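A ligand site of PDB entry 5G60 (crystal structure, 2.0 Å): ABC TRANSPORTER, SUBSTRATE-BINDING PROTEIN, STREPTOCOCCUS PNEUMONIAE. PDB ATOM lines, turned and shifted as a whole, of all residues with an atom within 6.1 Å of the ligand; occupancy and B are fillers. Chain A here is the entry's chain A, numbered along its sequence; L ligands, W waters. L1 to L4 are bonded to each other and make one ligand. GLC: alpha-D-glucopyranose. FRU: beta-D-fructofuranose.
Water W3 lies within hydrogen-bond range of an oxygen (O4) of FRU L3, the side-chain carboxylate of Asp 271 and the side-chain carboxylate of Asp 400.
Water W9 lies within hydrogen-bond range of O6 of FRU L4 (2.6 Å), O of Asp 400 (2.9 Å) and OD2 of Asp 271 (3.0 Å).
Water W2 lies within hydrogen-bond range of an oxygen (O4) of FRU L4 (2.7 Å) and the side-chain carboxylate of Asp 400 (2.8 Å).
Water W5 bridges O5 of FRU L3 (2.9 Å) and ND2 of Asn 191 (3.1 Å).
Water W8 lies within hydrogen-bond range of the side-chain carboxylate (OE2) of Glu 192, an oxygen (O6) of FRU L3 and the side-chain amide nitrogen (ND2) of Asn 191.
Water W4 lies within hydrogen-bond range of the guanidinium group of Arg 375 and an oxygen (O1) of FRU L4.
The side-chain carboxylate of Glu 379 is in salt-bridge range of the guanidinium group of Arg 375, 3.0 Å away.
The guanidinium group of Arg 375 is in hydrogen-bond range of the backbone carbonyl oxygen of Asn 339, at 3.0 Å.
The backbone carbonyl oxygen (O) of Lys 309 lies within hydrogen-bond range of the backbone NH (N) of Asn 64 (2.7 Å).
ND2 of Asn 339 lies close to NE1 of Trp 340, 3.2 Å away.
OG of Ser 12 is in hydrogen-bond range of OE1 of Gln 376, at 2.5 Å.
O of Ala 372 lies within hydrogen-bond range of NE2 of Gln 376 (3.2 Å).
The side-chain carboxylate (OE2) of Glu 123 is in hydrogen-bond range of the side-chain amide nitrogen (ND2) of Asn 339 (2.9 Å).
The backbone NH (N) of Ile 132 sits at hydrogen-bond distance from the backbone carbonyl oxygen (O) of Leu 125, 3.1 Å away.
The side-chain amide nitrogen of Asn 191 is in hydrogen-bond range of an oxygen (O6) of FRU L3.
NH1 of Arg 375 is in hydrogen-bond range of O3 of FRU L3.
The side-chain carboxylate (OE2) of Glu 123 lies within hydrogen-bond range of an oxygen (O3) of FRU L4 (2.6 Å).
An oxygen (O3) of FRU L4 sits at hydrogen-bond distance from the indole nitrogen (NE1) of Trp 340 (2.9 Å).
An oxygen (O4) of FRU L2 is in hydrogen-bond range of the backbone NH (N) of Gln 376 (3.4 Å).
An oxygen (O6) of FRU L4 is in hydrogen-bond range of the indole nitrogen of Trp 270 (3.0 Å).
O4 of FRU L2 sits at hydrogen-bond distance from OE2 of Glu 379 (2.5 Å).
O4 of FRU L3 lies within hydrogen-bond range of ND2 of Asn 274, at 2.8 Å.
Merely in contact with the ligand: Ala 401 (3.5 Å), Arg 404 (3.6 Å), Pro 398 (3.6 Å), Ile 132 (3.7 Å), Ala 372 (3.7 Å), Asp 400 (3.8 Å), His 133 (3.8 Å), Lys 309 (3.8 Å), Trp 121 (3.8 Å), Pro 371 (3.9 Å) and Leu 125 (3.9 Å).
Within 4 Å of the ligand: Trp 121, Glu 123, Leu 125, Ile 132, His 133, Asn 191, Trp 270, Asn 274, Lys 309, Trp 340, Pro 371, Ala 372, Arg 375, Gln 376, Glu 379, Pro 398, Asp 400, Ala 401 and Arg 404.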
ATOM      1  N   SER A  12      20.286  -3.747 -14.401  1.00  0.00           N
ATOM      2  CA  SER A  12      19.093  -3.336 -13.684  1.00  0.00           C
ATOM      3  C   SER A  12      18.874  -4.260 -12.500  1.00  0.00           C
ATOM      4  O   SER A  12      19.064  -5.461 -12.650  1.00  0.00           O
ATOM      5  CB  SER A  12      17.864  -3.430 -14.597  1.00  0.00           C
ATOM      6  OG  SER A  12      16.657  -3.448 -13.808  1.00  0.00           O
ATOM      7  N   ASN A  64      29.663  -2.487 -20.016  1.00  0.00           N
ATOM      8  CA  ASN A  64      28.524  -1.558 -19.787  1.00  0.00           C
ATOM      9  C   ASN A  64      28.839  -0.398 -18.824  1.00  0.00           C
ATOM     10  O   ASN A  64      28.019   0.066 -18.050  1.00  0.00           O
ATOM     11  CB  ASN A  64      27.282  -2.339 -19.318  1.00  0.00           C
ATOM     12  CG  ASN A  64      25.969  -1.650 -19.680  1.00  0.00           C
ATOM     13  OD1 ASN A  64      25.811  -1.044 -20.775  1.00  0.00           O
ATOM     14  ND2 ASN A  64      25.013  -1.784 -18.814  1.00  0.00           N
ATOM     15  N   TRP A 121      28.753   2.255 -27.794  1.00  0.00           N
ATOM     16  CA  TRP A 121      27.392   1.907 -28.074  1.00  0.00           C
ATOM     17  C   TRP A 121      26.949   2.873 -29.160  1.00  0.00           C
ATOM     18  O   TRP A 121      27.167   4.086 -29.062  1.00  0.00           O
ATOM     19  CB  TRP A 121      26.550   2.085 -26.768  1.00  0.00           C
ATOM     20  CG  TRP A 121      25.065   2.019 -26.869  1.00  0.00           C
ATOM     21  CD1 TRP A 121      24.278   0.877 -26.858  1.00  0.00           C
ATOM     22  CD2 TRP A 121      24.155   3.123 -27.019  1.00  0.00           C
ATOM     23  NE1 TRP A 121      22.942   1.225 -26.992  1.00  0.00           N
ATOM     24  CE2 TRP A 121      22.854   2.598 -27.067  1.00  0.00           C
ATOM     25  CE3 TRP A 121      24.329   4.499 -27.096  1.00  0.00           C
ATOM     26  CZ2 TRP A 121      21.722   3.406 -27.206  1.00  0.00           C
ATOM     27  CZ3 TRP A 121      23.202   5.300 -27.186  1.00  0.00           C
ATOM     28  CH2 TRP A 121      21.907   4.746 -27.248  1.00  0.00           C
ATOM     29  N   GLU A 123      23.573   3.545 -31.665  1.00  0.00           N
ATOM     30  CA  GLU A 123      22.211   3.238 -31.987  1.00  0.00           C
ATOM     31  C   GLU A 123      21.665   4.395 -32.818  1.00  0.00           C
ATOM     32  O   GLU A 123      21.450   5.491 -32.308  1.00  0.00           O
ATOM     33  CB  GLU A 123      21.443   3.078 -30.705  1.00  0.00           C
ATOM     34  CG  GLU A 123      19.956   2.749 -30.838  1.00  0.00           C
ATOM     35  CD  GLU A 123      19.239   2.997 -29.538  1.00  0.00           C
ATOM     36  OE1 GLU A 123      18.949   4.158 -29.242  1.00  0.00           O
ATOM     37  OE2 GLU A 123      19.019   2.035 -28.765  1.00  0.00           O
ATOM     38  N   LEU A 125      18.846   6.212 -34.559  1.00  0.00           N
ATOM     39  CA  LEU A 125      17.411   6.451 -34.477  1.00  0.00           C
ATOM     40  C   LEU A 125      17.217   7.965 -34.622  1.00  0.00           C
ATOM     41  O   LEU A 125      17.334   8.721 -33.628  1.00  0.00           O
ATOM     42  CB  LEU A 125      16.825   5.953 -33.137  1.00  0.00           C
ATOM     43  CG  LEU A 125      16.804   4.448 -32.937  1.00  0.00           C
ATOM     44  CD1 LEU A 125      16.472   3.991 -31.493  1.00  0.00           C
ATOM     45  CD2 LEU A 125      15.810   3.853 -33.951  1.00  0.00           C
ATOM     46  N   ILE A 132      16.046  10.821 -31.802  1.00  0.00           N
ATOM     47  CA  ILE A 132      15.171  10.389 -30.698  1.00  0.00           C
ATOM     48  C   ILE A 132      15.623  11.008 -29.357  1.00  0.00           C
ATOM     49  O   ILE A 132      14.812  11.155 -28.444  1.00  0.00           O
ATOM     50  CB  ILE A 132      15.108   8.856 -30.607  1.00  0.00           C
ATOM     51  CG1 ILE A 132      13.894   8.421 -29.777  1.00  0.00           C
ATOM     52  CG2 ILE A 132      16.390   8.295 -30.024  1.00  0.00           C
ATOM     53  CD1 ILE A 132      13.601   6.929 -29.921  1.00  0.00           C
ATOM     54  N   HIS A 133      16.898  11.380 -29.262  1.00  0.00           N
ATOM     55  CA  HIS A 133      17.486  12.014 -28.090  1.00  0.00           C
ATOM     56  C   HIS A 133      17.240  13.531 -27.924  1.00  0.00           C
ATOM     57  O   HIS A 133      17.522  14.107 -26.857  1.00  0.00           O
ATOM     58  CB  HIS A 133      18.977  11.745 -28.091  1.00  0.00           C
ATOM     59  CG  HIS A 133      19.297  10.302 -28.173  1.00  0.00           C
ATOM     60  ND1 HIS A 133      19.277   9.475 -27.080  1.00  0.00           N
ATOM     61  CD2 HIS A 133      19.553   9.511 -29.237  1.00  0.00           C
ATOM     62  CE1 HIS A 133      19.576   8.241 -27.446  1.00  0.00           C
ATOM     63  NE2 HIS A 133      19.716   8.240 -28.759  1.00  0.00           N
ATOM     64  N   ASN A 191      14.852  11.944 -17.378  1.00  0.00           N
ATOM     65  CA  ASN A 191      13.682  11.969 -18.178  1.00  0.00           C
ATOM     66  C   ASN A 191      12.472  12.431 -17.481  1.00  0.00           C
ATOM     67  O   ASN A 191      11.478  12.730 -18.116  1.00  0.00           O
ATOM     68  CB  ASN A 191      13.377  10.561 -18.727  1.00  0.00           C
ATOM     69  CG  ASN A 191      14.489  10.005 -19.541  1.00  0.00           C
ATOM     70  OD1 ASN A 191      15.345  10.729 -20.001  1.00  0.00           O
ATOM     71  ND2 ASN A 191      14.476   8.697 -19.735  1.00  0.00           N
ATOM     72  N   GLU A 192      12.531  12.517 -16.159  1.00  0.00           N
ATOM     73  CA  GLU A 192      11.342  12.902 -15.385  1.00  0.00           C
ATOM     74  C   GLU A 192      11.418  14.340 -14.829  1.00  0.00           C
ATOM     75  O   GLU A 192      10.526  14.771 -14.155  1.00  0.00           O
ATOM     76  CB  GLU A 192      11.098  11.871 -14.275  1.00  0.00           C
ATOM     77  CG  GLU A 192      10.590  10.514 -14.770  1.00  0.00           C
ATOM     78  CD  GLU A 192      11.597   9.739 -15.572  1.00  0.00           C
ATOM     79  OE1 GLU A 192      12.798   9.661 -15.158  1.00  0.00           O
ATOM     80  OE2 GLU A 192      11.187   9.193 -16.620  1.00  0.00           O
ATOM     81  N   TRP A 252      11.530   6.959  -8.474  1.00  0.00           N
ATOM     82  CA  TRP A 252      10.924   6.341  -9.631  1.00  0.00           C
ATOM     83  C   TRP A 252       9.808   5.350  -9.271  1.00  0.00           C
ATOM     84  O   TRP A 252       8.692   5.390  -9.820  1.00  0.00           O
ATOM     85  CB  TRP A 252      12.020   5.665 -10.421  1.00  0.00           C
ATOM     86  CG  TRP A 252      11.600   4.947 -11.664  1.00  0.00           C
ATOM     87  CD1 TRP A 252      11.741   3.606 -11.908  1.00  0.00           C
ATOM     88  CD2 TRP A 252      10.977   5.499 -12.842  1.00  0.00           C
ATOM     89  NE1 TRP A 252      11.240   3.290 -13.149  1.00  0.00           N
ATOM     90  CE2 TRP A 252      10.783   4.430 -13.761  1.00  0.00           C
ATOM     91  CE3 TRP A 252      10.552   6.784 -13.217  1.00  0.00           C
ATOM     92  CZ2 TRP A 252      10.195   4.610 -15.022  1.00  0.00           C
ATOM     93  CZ3 TRP A 252       9.966   6.963 -14.464  1.00  0.00           C
ATOM     94  CH2 TRP A 252       9.804   5.879 -15.358  1.00  0.00           C
ATOM     95  N   TRP A 270      10.152   9.716 -20.365  1.00  0.00           N
ATOM     96  CA  TRP A 270      10.586   9.395 -21.730  1.00  0.00           C
ATOM     97  C   TRP A 270       9.421   8.907 -22.608  1.00  0.00           C
ATOM     98  O   TRP A 270       9.235   9.350 -23.761  1.00  0.00           O
ATOM     99  CB  TRP A 270      11.736   8.420 -21.697  1.00  0.00           C
ATOM    100  CG  TRP A 270      12.248   8.016 -23.018  1.00  0.00           C
ATOM    101  CD1 TRP A 270      11.740   7.023 -23.802  1.00  0.00           C
ATOM    102  CD2 TRP A 270      13.350   8.541 -23.704  1.00  0.00           C
ATOM    103  NE1 TRP A 270      12.481   6.890 -24.935  1.00  0.00           N
ATOM    104  CE2 TRP A 270      13.486   7.811 -24.914  1.00  0.00           C
ATOM    105  CE3 TRP A 270      14.286   9.543 -23.422  1.00  0.00           C
ATOM    106  CZ2 TRP A 270      14.485   8.082 -25.871  1.00  0.00           C
ATOM    107  CZ3 TRP A 270      15.296   9.793 -24.344  1.00  0.00           C
ATOM    108  CH2 TRP A 270      15.382   9.067 -25.550  1.00  0.00           C
ATOM    109  N   ASP A 271       8.660   7.973 -22.048  1.00  0.00           N
ATOM    110  CA  ASP A 271       7.572   7.320 -22.725  1.00  0.00           C
ATOM    111  C   ASP A 271       6.490   7.035 -21.682  1.00  0.00           C
ATOM    112  O   ASP A 271       6.761   6.334 -20.710  1.00  0.00           O
ATOM    113  CB  ASP A 271       8.155   6.046 -23.359  1.00  0.00           C
ATOM    114  CG  ASP A 271       7.150   5.147 -24.041  1.00  0.00           C
ATOM    115  OD1 ASP A 271       5.915   5.343 -23.934  1.00  0.00           O
ATOM    116  OD2 ASP A 271       7.652   4.162 -24.685  1.00  0.00           O
ATOM    117  N   ASN A 274       5.693   3.607 -19.763  1.00  0.00           N
ATOM    118  CA  ASN A 274       6.418   3.204 -18.583  1.00  0.00           C
ATOM    119  C   ASN A 274       5.811   3.713 -17.282  1.00  0.00           C
ATOM    120  O   ASN A 274       6.193   3.218 -16.253  1.00  0.00           O
ATOM    121  CB  ASN A 274       7.864   3.694 -18.683  1.00  0.00           C
ATOM    122  CG  ASN A 274       8.636   3.028 -19.819  1.00  0.00           C
ATOM    123  OD1 ASN A 274       8.398   1.840 -20.142  1.00  0.00           O
ATOM    124  ND2 ASN A 274       9.583   3.757 -20.387  1.00  0.00           N
ATOM    125  N   LYS A 309      31.173   1.908 -23.478  1.00  0.00           N
ATOM    126  CA  LYS A 309      30.442   0.795 -22.883  1.00  0.00           C
ATOM    127  C   LYS A 309      31.347  -0.419 -22.589  1.00  0.00           C
ATOM    128  O   LYS A 309      30.837  -1.475 -22.264  1.00  0.00           O
ATOM    129  CB  LYS A 309      29.197   0.464 -23.664  1.00  0.00           C
ATOM    130  CG  LYS A 309      28.130   1.556 -23.543  1.00  0.00           C
ATOM    131  CD  LYS A 309      27.570   1.738 -22.129  1.00  0.00           C
ATOM    132  CE  LYS A 309      26.685   2.981 -22.020  1.00  0.00           C
ATOM    133  NZ  LYS A 309      25.534   2.748 -21.106  1.00  0.00           N
ATOM    134  N   ASN A 339      21.185  -5.027 -27.104  1.00  0.00           N
ATOM    135  CA  ASN A 339      20.544  -3.771 -26.862  1.00  0.00           C
ATOM    136  C   ASN A 339      19.154  -3.881 -26.353  1.00  0.00           C
ATOM    137  O   ASN A 339      18.751  -3.125 -25.431  1.00  0.00           O
ATOM    138  CB  ASN A 339      20.510  -2.908 -28.128  1.00  0.00           C
ATOM    139  CG  ASN A 339      20.386  -1.439 -27.802  1.00  0.00           C
ATOM    140  OD1 ASN A 339      21.016  -0.925 -26.846  1.00  0.00           O
ATOM    141  ND2 ASN A 339      19.598  -0.767 -28.568  1.00  0.00           N
ATOM    142  N   TRP A 340      18.358  -4.696 -27.013  1.00  0.00           N
ATOM    143  CA  TRP A 340      16.892  -4.623 -26.812  1.00  0.00           C
ATOM    144  C   TRP A 340      16.229  -5.853 -26.151  1.00  0.00           C
ATOM    145  O   TRP A 340      15.108  -5.741 -25.628  1.00  0.00           O
ATOM    146  CB  TRP A 340      16.248  -4.292 -28.149  1.00  0.00           C
ATOM    147  CG  TRP A 340      16.375  -2.828 -28.585  1.00  0.00           C
ATOM    148  CD1 TRP A 340      16.351  -1.711 -27.767  1.00  0.00           C
ATOM    149  CD2 TRP A 340      16.487  -2.332 -29.931  1.00  0.00           C
ATOM    150  NE1 TRP A 340      16.424  -0.555 -28.543  1.00  0.00           N
ATOM    151  CE2 TRP A 340      16.536  -0.916 -29.870  1.00  0.00           C
ATOM    152  CE3 TRP A 340      16.557  -2.951 -31.186  1.00  0.00           C
ATOM    153  CZ2 TRP A 340      16.658  -0.118 -31.021  1.00  0.00           C
ATOM    154  CZ3 TRP A 340      16.711  -2.127 -32.341  1.00  0.00           C
ATOM    155  CH2 TRP A 340      16.752  -0.738 -32.236  1.00  0.00           C
ATOM    156  N   PRO A 371       7.497  -1.039 -21.936  1.00  0.00           N
ATOM    157  CA  PRO A 371       8.739  -1.108 -22.713  1.00  0.00           C
ATOM    158  C   PRO A 371       9.977  -1.371 -21.867  1.00  0.00           C
ATOM    159  O   PRO A 371      10.608  -2.368 -21.983  1.00  0.00           O
ATOM    160  CB  PRO A 371       8.829   0.283 -23.386  1.00  0.00           C
ATOM    161  CG  PRO A 371       7.440   0.849 -23.391  1.00  0.00           C
ATOM    162  CD  PRO A 371       6.641   0.127 -22.319  1.00  0.00           C
ATOM    163  N   ALA A 372      10.288  -0.432 -20.992  1.00  0.00           N
ATOM    164  CA  ALA A 372      11.517  -0.475 -20.198  1.00  0.00           C
ATOM    165  C   ALA A 372      11.602  -1.710 -19.280  1.00  0.00           C
ATOM    166  O   ALA A 372      12.705  -2.138 -18.995  1.00  0.00           O
ATOM    167  CB  ALA A 372      11.618   0.790 -19.351  1.00  0.00           C
ATOM    168  N   GLU A 373      10.457  -2.251 -18.831  1.00  0.00           N
ATOM    169  CA  GLU A 373      10.445  -3.372 -17.856  1.00  0.00           C
ATOM    170  C   GLU A 373      11.037  -4.686 -18.363  1.00  0.00           C
ATOM    171  O   GLU A 373      11.983  -5.209 -17.748  1.00  0.00           O
ATOM    172  CB  GLU A 373       9.044  -3.644 -17.337  1.00  0.00           C
ATOM    173  CG  GLU A 373       9.010  -4.618 -16.177  1.00  0.00           C
ATOM    174  CD  GLU A 373       7.576  -4.905 -15.782  1.00  0.00           C
ATOM    175  OE1 GLU A 373       6.865  -3.939 -15.416  1.00  0.00           O
ATOM    176  OE2 GLU A 373       7.154  -6.076 -15.933  1.00  0.00           O
ATOM    177  N   ARG A 375      12.742  -5.119 -21.131  1.00  0.00           N
ATOM    178  CA  ARG A 375      14.057  -4.784 -21.657  1.00  0.00           C
ATOM    179  C   ARG A 375      15.133  -4.903 -20.599  1.00  0.00           C
ATOM    180  O   ARG A 375      16.121  -5.636 -20.774  1.00  0.00           O
ATOM    181  CB  ARG A 375      14.025  -3.341 -22.263  1.00  0.00           C
ATOM    182  CG  ARG A 375      15.360  -2.930 -22.856  1.00  0.00           C
ATOM    183  CD  ARG A 375      15.375  -1.590 -23.522  1.00  0.00           C
ATOM    184  NE  ARG A 375      16.726  -1.356 -24.021  1.00  0.00           N
ATOM    185  CZ  ARG A 375      17.139  -0.257 -24.665  1.00  0.00           C
ATOM    186  NH1 ARG A 375      16.306   0.748 -24.884  1.00  0.00           N
ATOM    187  NH2 ARG A 375      18.392  -0.186 -25.110  1.00  0.00           N
ATOM    188  N   GLN A 376      14.935  -4.221 -19.474  1.00  0.00           N
ATOM    189  CA  GLN A 376      15.928  -4.228 -18.431  1.00  0.00           C
ATOM    190  C   GLN A 376      16.188  -5.602 -17.804  1.00  0.00           C
ATOM    191  O   GLN A 376      17.284  -5.854 -17.293  1.00  0.00           O
ATOM    192  CB  GLN A 376      15.682  -3.091 -17.422  1.00  0.00           C
ATOM    193  CG  GLN A 376      14.526  -3.273 -16.501  1.00  0.00           C
ATOM    194  CD  GLN A 376      14.313  -2.028 -15.653  1.00  0.00           C
ATOM    195  OE1 GLN A 376      14.913  -1.887 -14.624  1.00  0.00           O
ATOM    196  NE2 GLN A 376      13.391  -1.170 -16.068  1.00  0.00           N
ATOM    197  N   LYS A 377      15.209  -6.491 -17.892  1.00  0.00           N
ATOM    198  CA  LYS A 377      15.381  -7.907 -17.527  1.00  0.00           C
ATOM    199  C   LYS A 377      16.194  -8.716 -18.537  1.00  0.00           C
ATOM    200  O   LYS A 377      16.952  -9.591 -18.149  1.00  0.00           O
ATOM    201  CB  LYS A 377      13.992  -8.563 -17.323  1.00  0.00           C
ATOM    202  CG  LYS A 377      13.215  -8.015 -16.150  1.00  0.00           C
ATOM    203  CD  LYS A 377      11.832  -8.633 -16.132  1.00  0.00           C
ATOM    204  CE  LYS A 377      11.033  -8.105 -14.963  1.00  0.00           C
ATOM    205  NZ  LYS A 377       9.569  -8.380 -15.113  1.00  0.00           N
ATOM    206  N   GLU A 379      17.942  -7.387 -21.688  1.00  0.00           N
ATOM    207  CA  GLU A 379      19.059  -6.786 -22.384  1.00  0.00           C
ATOM    208  C   GLU A 379      20.361  -7.098 -21.671  1.00  0.00           C
ATOM    209  O   GLU A 379      20.372  -7.579 -20.522  1.00  0.00           O
ATOM    210  CB  GLU A 379      18.870  -5.243 -22.487  1.00  0.00           C
ATOM    211  CG  GLU A 379      19.129  -4.497 -21.157  1.00  0.00           C
ATOM    212  CD  GLU A 379      18.764  -3.017 -21.150  1.00  0.00           C
ATOM    213  OE1 GLU A 379      18.862  -2.280 -22.193  1.00  0.00           O
ATOM    214  OE2 GLU A 379      18.387  -2.585 -20.027  1.00  0.00           O
ATOM    215  N   PRO A 398      12.016  -0.780 -33.424  1.00  0.00           N
ATOM    216  CA  PRO A 398      11.010  -0.864 -32.369  1.00  0.00           C
ATOM    217  C   PRO A 398       9.824   0.045 -32.632  1.00  0.00           C
ATOM    218  O   PRO A 398      10.011   1.186 -33.035  1.00  0.00           O
ATOM    219  CB  PRO A 398      11.757  -0.367 -31.125  1.00  0.00           C
ATOM    220  CG  PRO A 398      13.213  -0.604 -31.415  1.00  0.00           C
ATOM    221  CD  PRO A 398      13.348  -0.438 -32.900  1.00  0.00           C
ATOM    222  N   ASP A 400       7.875   1.378 -30.379  1.00  0.00           N
ATOM    223  CA  ASP A 400       7.906   2.495 -29.410  1.00  0.00           C
ATOM    224  C   ASP A 400       8.909   3.584 -29.881  1.00  0.00           C
ATOM    225  O   ASP A 400       8.620   4.741 -29.785  1.00  0.00           O
ATOM    226  CB  ASP A 400       8.123   1.991 -27.982  1.00  0.00           C
ATOM    227  CG  ASP A 400       9.449   1.269 -27.777  1.00  0.00           C
ATOM    228  OD1 ASP A 400      10.115   0.883 -28.750  1.00  0.00           O
ATOM    229  OD2 ASP A 400       9.819   1.104 -26.595  1.00  0.00           O
ATOM    230  N   ALA A 401      10.035   3.187 -30.458  1.00  0.00           N
ATOM    231  CA  ALA A 401      11.013   4.126 -31.074  1.00  0.00           C
ATOM    232  C   ALA A 401      10.456   4.914 -32.261  1.00  0.00           C
ATOM    233  O   ALA A 401      10.549   6.147 -32.336  1.00  0.00           O
ATOM    234  CB  ALA A 401      12.256   3.362 -31.507  1.00  0.00           C
ATOM    235  N   ARG A 404       7.904   7.362 -30.989  1.00  0.00           N
ATOM    236  CA  ARG A 404       8.568   8.532 -30.400  1.00  0.00           C
ATOM    237  C   ARG A 404       9.210   9.457 -31.481  1.00  0.00           C
ATOM    238  O   ARG A 404       9.148  10.690 -31.386  1.00  0.00           O
ATOM    239  CB  ARG A 404       9.630   8.095 -29.357  1.00  0.00           C
ATOM    240  CG  ARG A 404       9.928   9.138 -28.270  1.00  0.00           C
ATOM    241  CD  ARG A 404      10.902   8.608 -27.232  1.00  0.00           C
ATOM    242  NE  ARG A 404      10.884   9.470 -26.049  1.00  0.00           N
ATOM    243  CZ  ARG A 404      11.627  10.549 -25.842  1.00  0.00           C
ATOM    244  NH1 ARG A 404      12.580  10.931 -26.718  1.00  0.00           N
ATOM    245  NH2 ARG A 404      11.420  11.259 -24.732  1.00  0.00           N
HETATM  246  C1  GLC L   1      18.678   4.021 -19.818  1.00  0.00           C
HETATM  247  C2  GLC L   1      20.105   4.476 -19.994  1.00  0.00           C
HETATM  248  C3  GLC L   1      21.028   3.575 -19.216  1.00  0.00           C
HETATM  249  C4  GLC L   1      20.633   3.605 -17.744  1.00  0.00           C
HETATM  250  C5  GLC L   1      19.176   3.180 -17.594  1.00  0.00           C
HETATM  251  C6  GLC L   1      18.655   3.324 -16.162  1.00  0.00           C
HETATM  252  O2  GLC L   1      20.421   4.397 -21.400  1.00  0.00           O
HETATM  253  O3  GLC L   1      22.391   3.953 -19.257  1.00  0.00           O
HETATM  254  O4  GLC L   1      21.528   2.705 -17.049  1.00  0.00           O
HETATM  255  O5  GLC L   1      18.304   3.941 -18.468  1.00  0.00           O
HETATM  256  O6  GLC L   1      19.349   4.311 -15.431  1.00  0.00           O
HETATM  257  C1  FRU L   2      16.963   3.210 -22.139  1.00  0.00           C
HETATM  258  C2  FRU L   2      17.343   2.335 -20.934  1.00  0.00           C
HETATM  259  C3  FRU L   2      17.404   0.814 -21.252  1.00  0.00           C
HETATM  260  C4  FRU L   2      16.830   0.158 -19.982  1.00  0.00           C
HETATM  261  C5  FRU L   2      15.798   1.239 -19.580  1.00  0.00           C
HETATM  262  C6  FRU L   2      15.366   1.193 -18.125  1.00  0.00           C
HETATM  263  O1  FRU L   2      15.720   2.727 -22.676  1.00  0.00           O
HETATM  264  O2  FRU L   2      18.544   2.695 -20.320  1.00  0.00           O
HETATM  265  O3  FRU L   2      18.714   0.289 -21.582  1.00  0.00           O
HETATM  266  O4  FRU L   2      16.280  -1.176 -20.189  1.00  0.00           O
HETATM  267  O5  FRU L   2      16.344   2.533 -19.926  1.00  0.00           O
HETATM  268  O6  FRU L   2      16.500   1.560 -17.377  1.00  0.00           O
HETATM  269  C1  FRU L   3      15.389   4.468 -24.352  1.00  0.00           C
HETATM  270  C2  FRU L   3      14.821   3.711 -23.151  1.00  0.00           C
HETATM  271  C3  FRU L   3      13.531   3.016 -23.475  1.00  0.00           C
HETATM  272  C4  FRU L   3      12.790   3.039 -22.156  1.00  0.00           C
HETATM  273  C5  FRU L   3      13.184   4.384 -21.572  1.00  0.00           C
HETATM  274  C6  FRU L   3      13.327   4.263 -20.049  1.00  0.00           C
HETATM  275  O1  FRU L   3      15.811   3.643 -25.438  1.00  0.00           O
HETATM  276  O3  FRU L   3      13.882   1.700 -23.867  1.00  0.00           O
HETATM  277  O4  FRU L   3      11.390   2.986 -22.329  1.00  0.00           O
HETATM  278  O5  FRU L   3      14.451   4.686 -22.157  1.00  0.00           O
HETATM  279  O6  FRU L   3      13.992   5.417 -19.545  1.00  0.00           O
HETATM  280  C1  FRU L   4      16.790   5.366 -26.882  1.00  0.00           C
HETATM  281  C2  FRU L   4      15.776   4.251 -26.729  1.00  0.00           C
HETATM  282  C3  FRU L   4      15.891   3.137 -27.755  1.00  0.00           C
HETATM  283  C4  FRU L   4      14.490   2.626 -27.801  1.00  0.00           C
HETATM  284  C5  FRU L   4      13.733   3.935 -27.769  1.00  0.00           C
HETATM  285  C6  FRU L   4      12.319   3.842 -27.201  1.00  0.00           C
HETATM  286  O1  FRU L   4      18.097   4.851 -26.714  1.00  0.00           O
HETATM  287  O3  FRU L   4      16.779   2.103 -27.355  1.00  0.00           O
HETATM  288  O4  FRU L   4      14.193   1.843 -28.969  1.00  0.00           O
HETATM  289  O5  FRU L   4      14.516   4.817 -26.973  1.00  0.00           O
HETATM  290  O6  FRU L   4      11.729   5.132 -27.192  1.00  0.00           O
HETATM  291  O   HOH W   1      15.927   5.057 -17.947  1.00  0.00           O
HETATM  292  O   HOH W   2      12.615  -0.110 -28.056  1.00  0.00           O
HETATM  293  O   HOH W   3      10.418   3.421 -24.573  1.00  0.00           O
HETATM  294  O   HOH W   4      19.157   2.512 -25.063  1.00  0.00           O
HETATM  295  O   HOH W   5      16.296   6.798 -21.308  1.00  0.00           O
HETATM  296  O   HOH W   6      19.373   5.985 -24.712  1.00  0.00           O
HETATM  297  O   HOH W   7      13.474   5.383 -16.754  1.00  0.00           O
HETATM  298  O   HOH W   8      12.110   7.369 -18.365  1.00  0.00           O
HETATM  299  O   HOH W   9       9.131   5.449 -27.008  1.00  0.00           O
